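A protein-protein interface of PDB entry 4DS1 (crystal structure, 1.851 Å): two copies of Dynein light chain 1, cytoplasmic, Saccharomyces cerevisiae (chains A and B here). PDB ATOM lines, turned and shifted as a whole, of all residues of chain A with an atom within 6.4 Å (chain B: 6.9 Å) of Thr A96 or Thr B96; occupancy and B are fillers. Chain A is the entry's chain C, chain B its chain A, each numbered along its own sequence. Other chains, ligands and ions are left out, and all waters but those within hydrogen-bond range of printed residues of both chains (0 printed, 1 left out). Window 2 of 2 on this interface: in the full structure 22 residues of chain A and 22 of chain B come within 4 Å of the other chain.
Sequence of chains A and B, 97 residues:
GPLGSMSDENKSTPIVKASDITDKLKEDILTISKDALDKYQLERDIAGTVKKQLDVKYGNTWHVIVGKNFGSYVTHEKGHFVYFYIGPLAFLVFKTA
Hydrophobic or aromatic side chains of chain A within 4 Å of the printed part of chain B: His A63 and Phe A94.
Hydrophobic or aromatic side chains of chain B that line the printed part of chain A: His B63 and Phe B94.
Thr A61 touches Thr B75, and with the chains exchanged Thr A75 touches Thr B61.
His A63 touches Phe B94, and with the chains exchanged Phe A94 touches His B63.
His A63 touches Thr B96, and with the chains exchanged Thr A96 touches His B63.
Thr B96 touches its own counterpart, Thr A96.
Of the 9 pairs that touch across the chains among the printed residues, 9 have their exchanged pair printed and touching as well.
A ring nitrogen (ND1) of His B63 lies within hydrogen-bond range of the backbone NH of Thr A75 (3.3 Å).
The backbone NH (N) of Thr B75 sits at hydrogen-bond distance from a ring nitrogen (ND1) of His A63 (3.2 Å).
The side-chain amide nitrogen (ND2) of Asn B60 sits close to the side-chain hydroxyl (OG1) of Thr B61.
The backbone carbonyl oxygen (O) of Thr B61 sits at hydrogen-bond distance from the backbone NH (N) of Thr B96.
O of Ala B97 sits at hydrogen-bond distance from OG1 of Thr B61 (2.7 Å).
NE2 of His B63 is in hydrogen-bond range of OG1 of Thr B96 (3.0 Å).
N of Thr A96 sits at hydrogen-bond distance from O of Thr A61, at 2.8 Å.
The backbone NH (N) of His A63 sits at hydrogen-bond distance from the backbone carbonyl oxygen (O) of Phe A94 (2.9 Å).
Thr A96 touches two residues of chain B.
Of chain A, only His A63 and Thr A96 come within 4 Å of Thr B96.
Printed residues of chain B within 4 Å of Thr A75: Thr B61 (3.4 Å) and His B63 (3.1 Å).
Of the printed residues of chain B, Phe A94 touches His B63 (3.8 Å).
Lys A95 touches none of the printed residues of chain B.
The nearest residue of chain A that does not touch Thr B96 is Ala A97 (4.1 Å).
CG2 of Thr A61 touches CB of Thr B75, at 3.3 Å.
CE2 of Phe B94 touches ND1 of His A63, at 3.7 Å.
Thr B96 touches His A63 (CG2 to CE1, 3.8 Å).
Thr B61 touches Thr A75 (CG2 to CB, 3.4 Å).
CE2 of Phe A94 touches ND1 of His B63, at 3.8 Å.
CE1 of His B63 touches CG2 of Thr A96, 3.6 Å away.
OG1 of Thr A96 touches OG1 of Thr B96, at 3.8 Å.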
ATOM      1  N   ASN A  60     -19.298 -13.720  -8.275  1.00  0.00           N
ATOM      2  CA  ASN A  60     -19.889 -13.037  -9.424  1.00  0.00           C
ATOM      3  C   ASN A  60     -19.745 -11.523  -9.252  1.00  0.00           C
ATOM      4  O   ASN A  60     -19.578 -11.045  -8.130  1.00  0.00           O
ATOM      5  CB  ASN A  60     -21.354 -13.444  -9.565  1.00  0.00           C
ATOM      6  CG  ASN A  60     -21.535 -14.954  -9.737  1.00  0.00           C
ATOM      7  OD1 ASN A  60     -20.742 -15.623 -10.411  1.00  0.00           O
ATOM      8  ND2 ASN A  60     -22.587 -15.491  -9.133  1.00  0.00           N
ATOM      9  N   THR A  61     -19.773 -10.750 -10.336  1.00  0.00           N
ATOM     10  CA  THR A  61     -19.987 -11.215 -11.697  1.00  0.00           C
ATOM     11  C   THR A  61     -18.873 -10.630 -12.567  1.00  0.00           C
ATOM     12  O   THR A  61     -18.672  -9.414 -12.587  1.00  0.00           O
ATOM     13  CB  THR A  61     -21.338 -10.687 -12.218  1.00  0.00           C
ATOM     14  OG1 THR A  61     -22.402 -11.209 -11.415  1.00  0.00           O
ATOM     15  CG2 THR A  61     -21.568 -11.087 -13.661  1.00  0.00           C
ATOM     16  N   TRP A  62     -18.161 -11.490 -13.283  1.00  0.00           N
ATOM     17  CA  TRP A  62     -17.038 -11.057 -14.104  1.00  0.00           C
ATOM     18  C   TRP A  62     -17.383 -11.018 -15.591  1.00  0.00           C
ATOM     19  O   TRP A  62     -18.297 -11.705 -16.053  1.00  0.00           O
ATOM     20  CB  TRP A  62     -15.825 -11.961 -13.869  1.00  0.00           C
ATOM     21  CG  TRP A  62     -15.235 -11.806 -12.488  1.00  0.00           C
ATOM     22  CD1 TRP A  62     -15.657 -12.426 -11.337  1.00  0.00           C
ATOM     23  CD2 TRP A  62     -14.128 -10.975 -12.116  1.00  0.00           C
ATOM     24  NE1 TRP A  62     -14.869 -12.033 -10.281  1.00  0.00           N
ATOM     25  CE2 TRP A  62     -13.926 -11.144 -10.733  1.00  0.00           C
ATOM     26  CE3 TRP A  62     -13.283 -10.106 -12.824  1.00  0.00           C
ATOM     27  CZ2 TRP A  62     -12.916 -10.471 -10.040  1.00  0.00           C
ATOM     28  CZ3 TRP A  62     -12.284  -9.446 -12.139  1.00  0.00           C
ATOM     29  CH2 TRP A  62     -12.104  -9.632 -10.761  1.00  0.00           C
ATOM     30  N   HIS A  63     -16.635 -10.209 -16.334  1.00  0.00           N
ATOM     31  CA  HIS A  63     -16.874 -10.044 -17.759  1.00  0.00           C
ATOM     32  C   HIS A  63     -15.518  -9.968 -18.429  1.00  0.00           C
ATOM     33  O   HIS A  63     -14.611  -9.306 -17.921  1.00  0.00           O
ATOM     34  CB  HIS A  63     -17.650  -8.755 -18.022  1.00  0.00           C
ATOM     35  CG  HIS A  63     -18.848  -8.587 -17.145  1.00  0.00           C
ATOM     36  ND1 HIS A  63     -20.106  -9.030 -17.504  1.00  0.00           N
ATOM     37  CD2 HIS A  63     -18.976  -8.036 -15.915  1.00  0.00           C
ATOM     38  CE1 HIS A  63     -20.958  -8.751 -16.531  1.00  0.00           C
ATOM     39  NE2 HIS A  63     -20.297  -8.151 -15.557  1.00  0.00           N
ATOM     40  N   THR A  75     -18.439  -0.019 -16.646  1.00  0.00           N
ATOM     41  CA  THR A  75     -18.358   0.366 -15.247  1.00  0.00           C
ATOM     42  C   THR A  75     -17.909  -0.864 -14.474  1.00  0.00           C
ATOM     43  O   THR A  75     -18.389  -1.962 -14.733  1.00  0.00           O
ATOM     44  CB  THR A  75     -19.722   0.840 -14.723  1.00  0.00           C
ATOM     45  OG1 THR A  75     -20.116   2.030 -15.419  1.00  0.00           O
ATOM     46  CG2 THR A  75     -19.662   1.114 -13.219  1.00  0.00           C
ATOM     47  N   HIS A  76     -16.972  -0.690 -13.545  1.00  0.00           N
ATOM     48  CA  HIS A  76     -16.471  -1.823 -12.771  1.00  0.00           C
ATOM     49  C   HIS A  76     -16.430  -1.504 -11.285  1.00  0.00           C
ATOM     50  O   HIS A  76     -16.316  -0.339 -10.897  1.00  0.00           O
ATOM     51  CB  HIS A  76     -15.073  -2.217 -13.241  1.00  0.00           C
ATOM     52  CG  HIS A  76     -14.060  -1.122 -13.105  1.00  0.00           C
ATOM     53  ND1 HIS A  76     -13.384  -0.875 -11.928  1.00  0.00           N
ATOM     54  CD2 HIS A  76     -13.605  -0.212 -13.998  1.00  0.00           C
ATOM     55  CE1 HIS A  76     -12.557   0.141 -12.104  1.00  0.00           C
ATOM     56  NE2 HIS A  76     -12.668   0.559 -13.353  1.00  0.00           N
ATOM     57  N   GLU A  77     -16.524  -2.540 -10.456  1.00  0.00           N
ATOM     58  CA  GLU A  77     -16.302  -2.364  -9.030  1.00  0.00           C
ATOM     59  C   GLU A  77     -14.893  -1.816  -8.856  1.00  0.00           C
ATOM     60  O   GLU A  77     -13.981  -2.199  -9.591  1.00  0.00           O
ATOM     61  CB  GLU A  77     -16.429  -3.697  -8.288  1.00  0.00           C
ATOM     62  CG  GLU A  77     -16.328  -3.516  -6.773  1.00  0.00           C
ATOM     63  CD  GLU A  77     -16.289  -4.824  -5.990  1.00  0.00           C
ATOM     64  OE1 GLU A  77     -16.621  -5.892  -6.551  1.00  0.00           O
ATOM     65  OE2 GLU A  77     -15.921  -4.767  -4.794  1.00  0.00           O
ATOM     66  N   HIS A  80     -11.332  -3.904  -9.079  1.00  0.00           N
ATOM     67  CA  HIS A  80     -11.576  -5.100  -9.879  1.00  0.00           C
ATOM     68  C   HIS A  80     -11.580  -4.819 -11.376  1.00  0.00           C
ATOM     69  O   HIS A  80     -12.562  -5.081 -12.067  1.00  0.00           O
ATOM     70  CB  HIS A  80     -12.880  -5.768  -9.439  1.00  0.00           C
ATOM     71  CG  HIS A  80     -12.832  -6.276  -8.032  1.00  0.00           C
ATOM     72  ND1 HIS A  80     -12.862  -5.435  -6.936  1.00  0.00           N
ATOM     73  CD2 HIS A  80     -12.704  -7.529  -7.539  1.00  0.00           C
ATOM     74  CE1 HIS A  80     -12.785  -6.154  -5.831  1.00  0.00           C
ATOM     75  NE2 HIS A  80     -12.685  -7.426  -6.170  1.00  0.00           N
ATOM     76  N   PHE A  94     -13.106  -7.459 -15.933  1.00  0.00           N
ATOM     77  CA  PHE A  94     -13.633  -6.632 -14.848  1.00  0.00           C
ATOM     78  C   PHE A  94     -14.837  -7.252 -14.171  1.00  0.00           C
ATOM     79  O   PHE A  94     -15.492  -8.142 -14.726  1.00  0.00           O
ATOM     80  CB  PHE A  94     -13.968  -5.222 -15.351  1.00  0.00           C
ATOM     81  CG  PHE A  94     -15.111  -5.176 -16.331  1.00  0.00           C
ATOM     82  CD1 PHE A  94     -14.922  -5.536 -17.656  1.00  0.00           C
ATOM     83  CD2 PHE A  94     -16.370  -4.754 -15.925  1.00  0.00           C
ATOM     84  CE1 PHE A  94     -15.967  -5.481 -18.559  1.00  0.00           C
ATOM     85  CE2 PHE A  94     -17.426  -4.700 -16.822  1.00  0.00           C
ATOM     86  CZ  PHE A  94     -17.223  -5.064 -18.142  1.00  0.00           C
ATOM     87  N   LYS A  95     -15.115  -6.763 -12.969  1.00  0.00           N
ATOM     88  CA  LYS A  95     -16.184  -7.295 -12.140  1.00  0.00           C
ATOM     89  C   LYS A  95     -17.271  -6.246 -11.933  1.00  0.00           C
ATOM     90  O   LYS A  95     -16.986  -5.043 -11.799  1.00  0.00           O
ATOM     91  CB  LYS A  95     -15.607  -7.736 -10.794  1.00  0.00           C
ATOM     92  CG  LYS A  95     -16.551  -8.570  -9.953  1.00  0.00           C
ATOM     93  CD  LYS A  95     -15.965  -8.773  -8.572  1.00  0.00           C
ATOM     94  CE  LYS A  95     -16.960  -9.434  -7.636  1.00  0.00           C
ATOM     95  NZ  LYS A  95     -16.512  -9.268  -6.220  1.00  0.00           N
ATOM     96  N   THR A  96     -18.519  -6.698 -11.926  1.00  0.00           N
ATOM     97  CA  THR A  96     -19.636  -5.827 -11.606  1.00  0.00           C
ATOM     98  C   THR A  96     -20.491  -6.475 -10.532  1.00  0.00           C
ATOM     99  O   THR A  96     -20.311  -7.652 -10.205  1.00  0.00           O
ATOM    100  CB  THR A  96     -20.545  -5.553 -12.830  1.00  0.00           C
ATOM    101  OG1 THR A  96     -21.242  -6.755 -13.195  1.00  0.00           O
ATOM    102  CG2 THR A  96     -19.728  -5.049 -14.010  1.00  0.00           C
ATOM    103  N   ALA A  97     -21.437  -5.706 -10.002  1.00  0.00           N
ATOM    104  CA  ALA A  97     -22.486  -6.266  -9.157  1.00  0.00           C
ATOM    105  C   ALA A  97     -23.357  -7.168 -10.010  1.00  0.00           C
ATOM    106  O   ALA A  97     -24.094  -8.027  -9.510  1.00  0.00           O
ATOM    107  CB  ALA A  97     -23.322  -5.151  -8.549  1.00  0.00           C
ATOM    108  OXT ALA A  97     -23.345  -7.034 -11.236  1.00  0.00           O
ATOM    109  N   GLY B  59     -31.309   3.901 -16.887  1.00  0.00           N
ATOM    110  CA  GLY B  59     -30.746   3.588 -15.587  1.00  0.00           C
ATOM    111  C   GLY B  59     -29.493   2.738 -15.718  1.00  0.00           C
ATOM    112  O   GLY B  59     -29.284   2.080 -16.730  1.00  0.00           O
ATOM    113  N   ASN B  60     -28.654   2.758 -14.688  1.00  0.00           N
ATOM    114  CA  ASN B  60     -27.414   1.997 -14.692  1.00  0.00           C
ATOM    115  C   ASN B  60     -27.714   0.499 -14.576  1.00  0.00           C
ATOM    116  O   ASN B  60     -28.803   0.127 -14.146  1.00  0.00           O
ATOM    117  CB  ASN B  60     -26.513   2.469 -13.550  1.00  0.00           C
ATOM    118  CG  ASN B  60     -27.216   2.442 -12.200  1.00  0.00           C
ATOM    119  OD1 ASN B  60     -27.739   3.457 -11.747  1.00  0.00           O
ATOM    120  ND2 ASN B  60     -27.224   1.279 -11.552  1.00  0.00           N
ATOM    121  N   THR B  61     -26.773  -0.368 -14.944  1.00  0.00           N
ATOM    122  CA  THR B  61     -25.433  -0.009 -15.394  1.00  0.00           C
ATOM    123  C   THR B  61     -25.189  -0.670 -16.743  1.00  0.00           C
ATOM    124  O   THR B  61     -25.255  -1.899 -16.846  1.00  0.00           O
ATOM    125  CB  THR B  61     -24.405  -0.583 -14.417  1.00  0.00           C
ATOM    126  OG1 THR B  61     -24.722  -0.146 -13.085  1.00  0.00           O
ATOM    127  CG2 THR B  61     -22.988  -0.149 -14.793  1.00  0.00           C
ATOM    128  N   TRP B  62     -24.886   0.123 -17.767  1.00  0.00           N
ATOM    129  CA  TRP B  62     -24.667  -0.429 -19.108  1.00  0.00           C
ATOM    130  C   TRP B  62     -23.183  -0.571 -19.430  1.00  0.00           C
ATOM    131  O   TRP B  62     -22.346   0.109 -18.840  1.00  0.00           O
ATOM    132  CB  TRP B  62     -25.363   0.433 -20.163  1.00  0.00           C
ATOM    133  CG  TRP B  62     -26.853   0.399 -20.049  1.00  0.00           C
ATOM    134  CD1 TRP B  62     -27.638   1.125 -19.190  1.00  0.00           C
ATOM    135  CD2 TRP B  62     -27.745  -0.406 -20.821  1.00  0.00           C
ATOM    136  NE1 TRP B  62     -28.961   0.814 -19.382  1.00  0.00           N
ATOM    137  CE2 TRP B  62     -29.055  -0.119 -20.382  1.00  0.00           C
ATOM    138  CE3 TRP B  62     -27.560  -1.337 -21.851  1.00  0.00           C
ATOM    139  CZ2 TRP B  62     -30.177  -0.736 -20.932  1.00  0.00           C
ATOM    140  CZ3 TRP B  62     -28.674  -1.948 -22.396  1.00  0.00           C
ATOM    141  CH2 TRP B  62     -29.967  -1.653 -21.932  1.00  0.00           C
ATOM    142  N   HIS B  63     -22.871  -1.450 -20.382  1.00  0.00           N
ATOM    143  CA  HIS B  63     -21.493  -1.699 -20.792  1.00  0.00           C
ATOM    144  C   HIS B  63     -21.510  -1.879 -22.290  1.00  0.00           C
ATOM    145  O   HIS B  63     -22.400  -2.537 -22.821  1.00  0.00           O
ATOM    146  CB  HIS B  63     -20.957  -2.964 -20.121  1.00  0.00           C
ATOM    147  CG  HIS B  63     -21.233  -3.017 -18.652  1.00  0.00           C
ATOM    148  ND1 HIS B  63     -20.363  -2.508 -17.710  1.00  0.00           N
ATOM    149  CD2 HIS B  63     -22.289  -3.511 -17.963  1.00  0.00           C
ATOM    150  CE1 HIS B  63     -20.877  -2.681 -16.502  1.00  0.00           C
ATOM    151  NE2 HIS B  63     -22.039  -3.296 -16.627  1.00  0.00           N
ATOM    152  N   THR B  75     -22.089 -11.369 -18.545  1.00  0.00           N
ATOM    153  CA  THR B  75     -23.335 -11.714 -17.882  1.00  0.00           C
ATOM    154  C   THR B  75     -24.229 -10.482 -17.926  1.00  0.00           C
ATOM    155  O   THR B  75     -23.766  -9.363 -17.671  1.00  0.00           O
ATOM    156  CB  THR B  75     -23.080 -12.124 -16.432  1.00  0.00           C
ATOM    157  OG1 THR B  75     -22.334 -13.349 -16.407  1.00  0.00           O
ATOM    158  CG2 THR B  75     -24.385 -12.316 -15.695  1.00  0.00           C
ATOM    159  N   HIS B  76     -25.498 -10.672 -18.269  1.00  0.00           N
ATOM    160  CA  HIS B  76     -26.392  -9.532 -18.445  1.00  0.00           C
ATOM    161  C   HIS B  76     -27.734  -9.743 -17.774  1.00  0.00           C
ATOM    162  O   HIS B  76     -28.199 -10.863 -17.622  1.00  0.00           O
ATOM    163  CB  HIS B  76     -26.622  -9.251 -19.933  1.00  0.00           C
ATOM    164  CG  HIS B  76     -27.335 -10.354 -20.653  1.00  0.00           C
ATOM    165  ND1 HIS B  76     -28.705 -10.515 -20.602  1.00  0.00           N
ATOM    166  CD2 HIS B  76     -26.868 -11.350 -21.442  1.00  0.00           C
ATOM    167  CE1 HIS B  76     -29.049 -11.564 -21.331  1.00  0.00           C
ATOM    168  NE2 HIS B  76     -27.952 -12.088 -21.850  1.00  0.00           N
ATOM    169  N   GLU B  77     -28.357  -8.642 -17.386  1.00  0.00           N
ATOM    170  CA  GLU B  77     -29.721  -8.673 -16.893  1.00  0.00           C
ATOM    171  C   GLU B  77     -30.643  -9.196 -17.988  1.00  0.00           C
ATOM    172  O   GLU B  77     -30.471  -8.885 -19.173  1.00  0.00           O
ATOM    173  CB  GLU B  77     -30.110  -7.260 -16.458  1.00  0.00           C
ATOM    174  CG  GLU B  77     -31.554  -7.048 -16.091  1.00  0.00           C
ATOM    175  CD  GLU B  77     -31.816  -5.603 -15.712  1.00  0.00           C
ATOM    176  OE1 GLU B  77     -30.925  -4.985 -15.085  1.00  0.00           O
ATOM    177  OE2 GLU B  77     -32.904  -5.088 -16.049  1.00  0.00           O
ATOM    178  N   HIS B  80     -31.871  -7.512 -21.490  1.00  0.00           N
ATOM    179  CA  HIS B  80     -31.011  -6.347 -21.709  1.00  0.00           C
ATOM    180  C   HIS B  80     -29.663  -6.701 -22.331  1.00  0.00           C
ATOM    181  O   HIS B  80     -28.605  -6.402 -21.768  1.00  0.00           O
ATOM    182  CB  HIS B  80     -30.817  -5.572 -20.403  1.00  0.00           C
ATOM    183  CG  HIS B  80     -32.078  -4.953 -19.884  1.00  0.00           C
ATOM    184  ND1 HIS B  80     -33.086  -5.693 -19.308  1.00  0.00           N
ATOM    185  CD2 HIS B  80     -32.503  -3.665 -19.875  1.00  0.00           C
ATOM    186  CE1 HIS B  80     -34.076  -4.889 -18.955  1.00  0.00           C
ATOM    187  NE2 HIS B  80     -33.746  -3.655 -19.290  1.00  0.00           N
ATOM    188  N   PHE B  94     -24.965  -4.289 -23.318  1.00  0.00           N
ATOM    189  CA  PHE B  94     -25.694  -5.006 -22.278  1.00  0.00           C
ATOM    190  C   PHE B  94     -25.736  -4.258 -20.951  1.00  0.00           C
ATOM    191  O   PHE B  94     -24.952  -3.332 -20.715  1.00  0.00           O
ATOM    192  CB  PHE B  94     -25.146  -6.424 -22.089  1.00  0.00           C
ATOM    193  CG  PHE B  94     -23.741  -6.479 -21.542  1.00  0.00           C
ATOM    194  CD1 PHE B  94     -22.644  -6.232 -22.360  1.00  0.00           C
ATOM    195  CD2 PHE B  94     -23.518  -6.821 -20.217  1.00  0.00           C
ATOM    196  CE1 PHE B  94     -21.350  -6.299 -21.851  1.00  0.00           C
ATOM    197  CE2 PHE B  94     -22.238  -6.896 -19.703  1.00  0.00           C
ATOM    198  CZ  PHE B  94     -21.146  -6.629 -20.521  1.00  0.00           C
ATOM    199  N   LYS B  95     -26.665  -4.679 -20.095  1.00  0.00           N
ATOM    200  CA  LYS B  95     -26.904  -4.032 -18.816  1.00  0.00           C
ATOM    201  C   LYS B  95     -26.712  -5.022 -17.678  1.00  0.00           C
ATOM    202  O   LYS B  95     -27.084  -6.194 -17.798  1.00  0.00           O
ATOM    203  CB  LYS B  95     -28.334  -3.476 -18.776  1.00  0.00           C
ATOM    204  CG  LYS B  95     -28.647  -2.610 -17.554  1.00  0.00           C
ATOM    205  CD  LYS B  95     -30.141  -2.263 -17.511  1.00  0.00           C
ATOM    206  CE  LYS B  95     -30.485  -1.482 -16.255  1.00  0.00           C
ATOM    207  NZ  LYS B  95     -30.211  -2.260 -15.003  1.00  0.00           N
ATOM    208  N   THR B  96     -26.122  -4.541 -16.584  1.00  0.00           N
ATOM    209  CA  THR B  96     -26.111  -5.253 -15.306  1.00  0.00           C
ATOM    210  C   THR B  96     -26.760  -4.362 -14.244  1.00  0.00           C
ATOM    211  O   THR B  96     -27.225  -3.264 -14.546  1.00  0.00           O
ATOM    212  CB  THR B  96     -24.685  -5.624 -14.846  1.00  0.00           C
ATOM    213  OG1 THR B  96     -23.918  -4.430 -14.611  1.00  0.00           O
ATOM    214  CG2 THR B  96     -23.974  -6.494 -15.905  1.00  0.00           C
ATOM    215  N   ALA B  97     -26.795  -4.830 -13.001  1.00  0.00           N
ATOM    216  CA  ALA B  97     -27.362  -4.031 -11.914  1.00  0.00           C
ATOM    217  C   ALA B  97     -26.741  -2.626 -11.880  1.00  0.00           C
ATOM    218  O   ALA B  97     -25.529  -2.464 -11.905  1.00  0.00           O
ATOM    219  CB  ALA B  97     -27.149  -4.737 -10.583  1.00  0.00           C
ATOM    220  OXT ALA B  97     -27.421  -1.603 -11.836  1.00  0.00           O
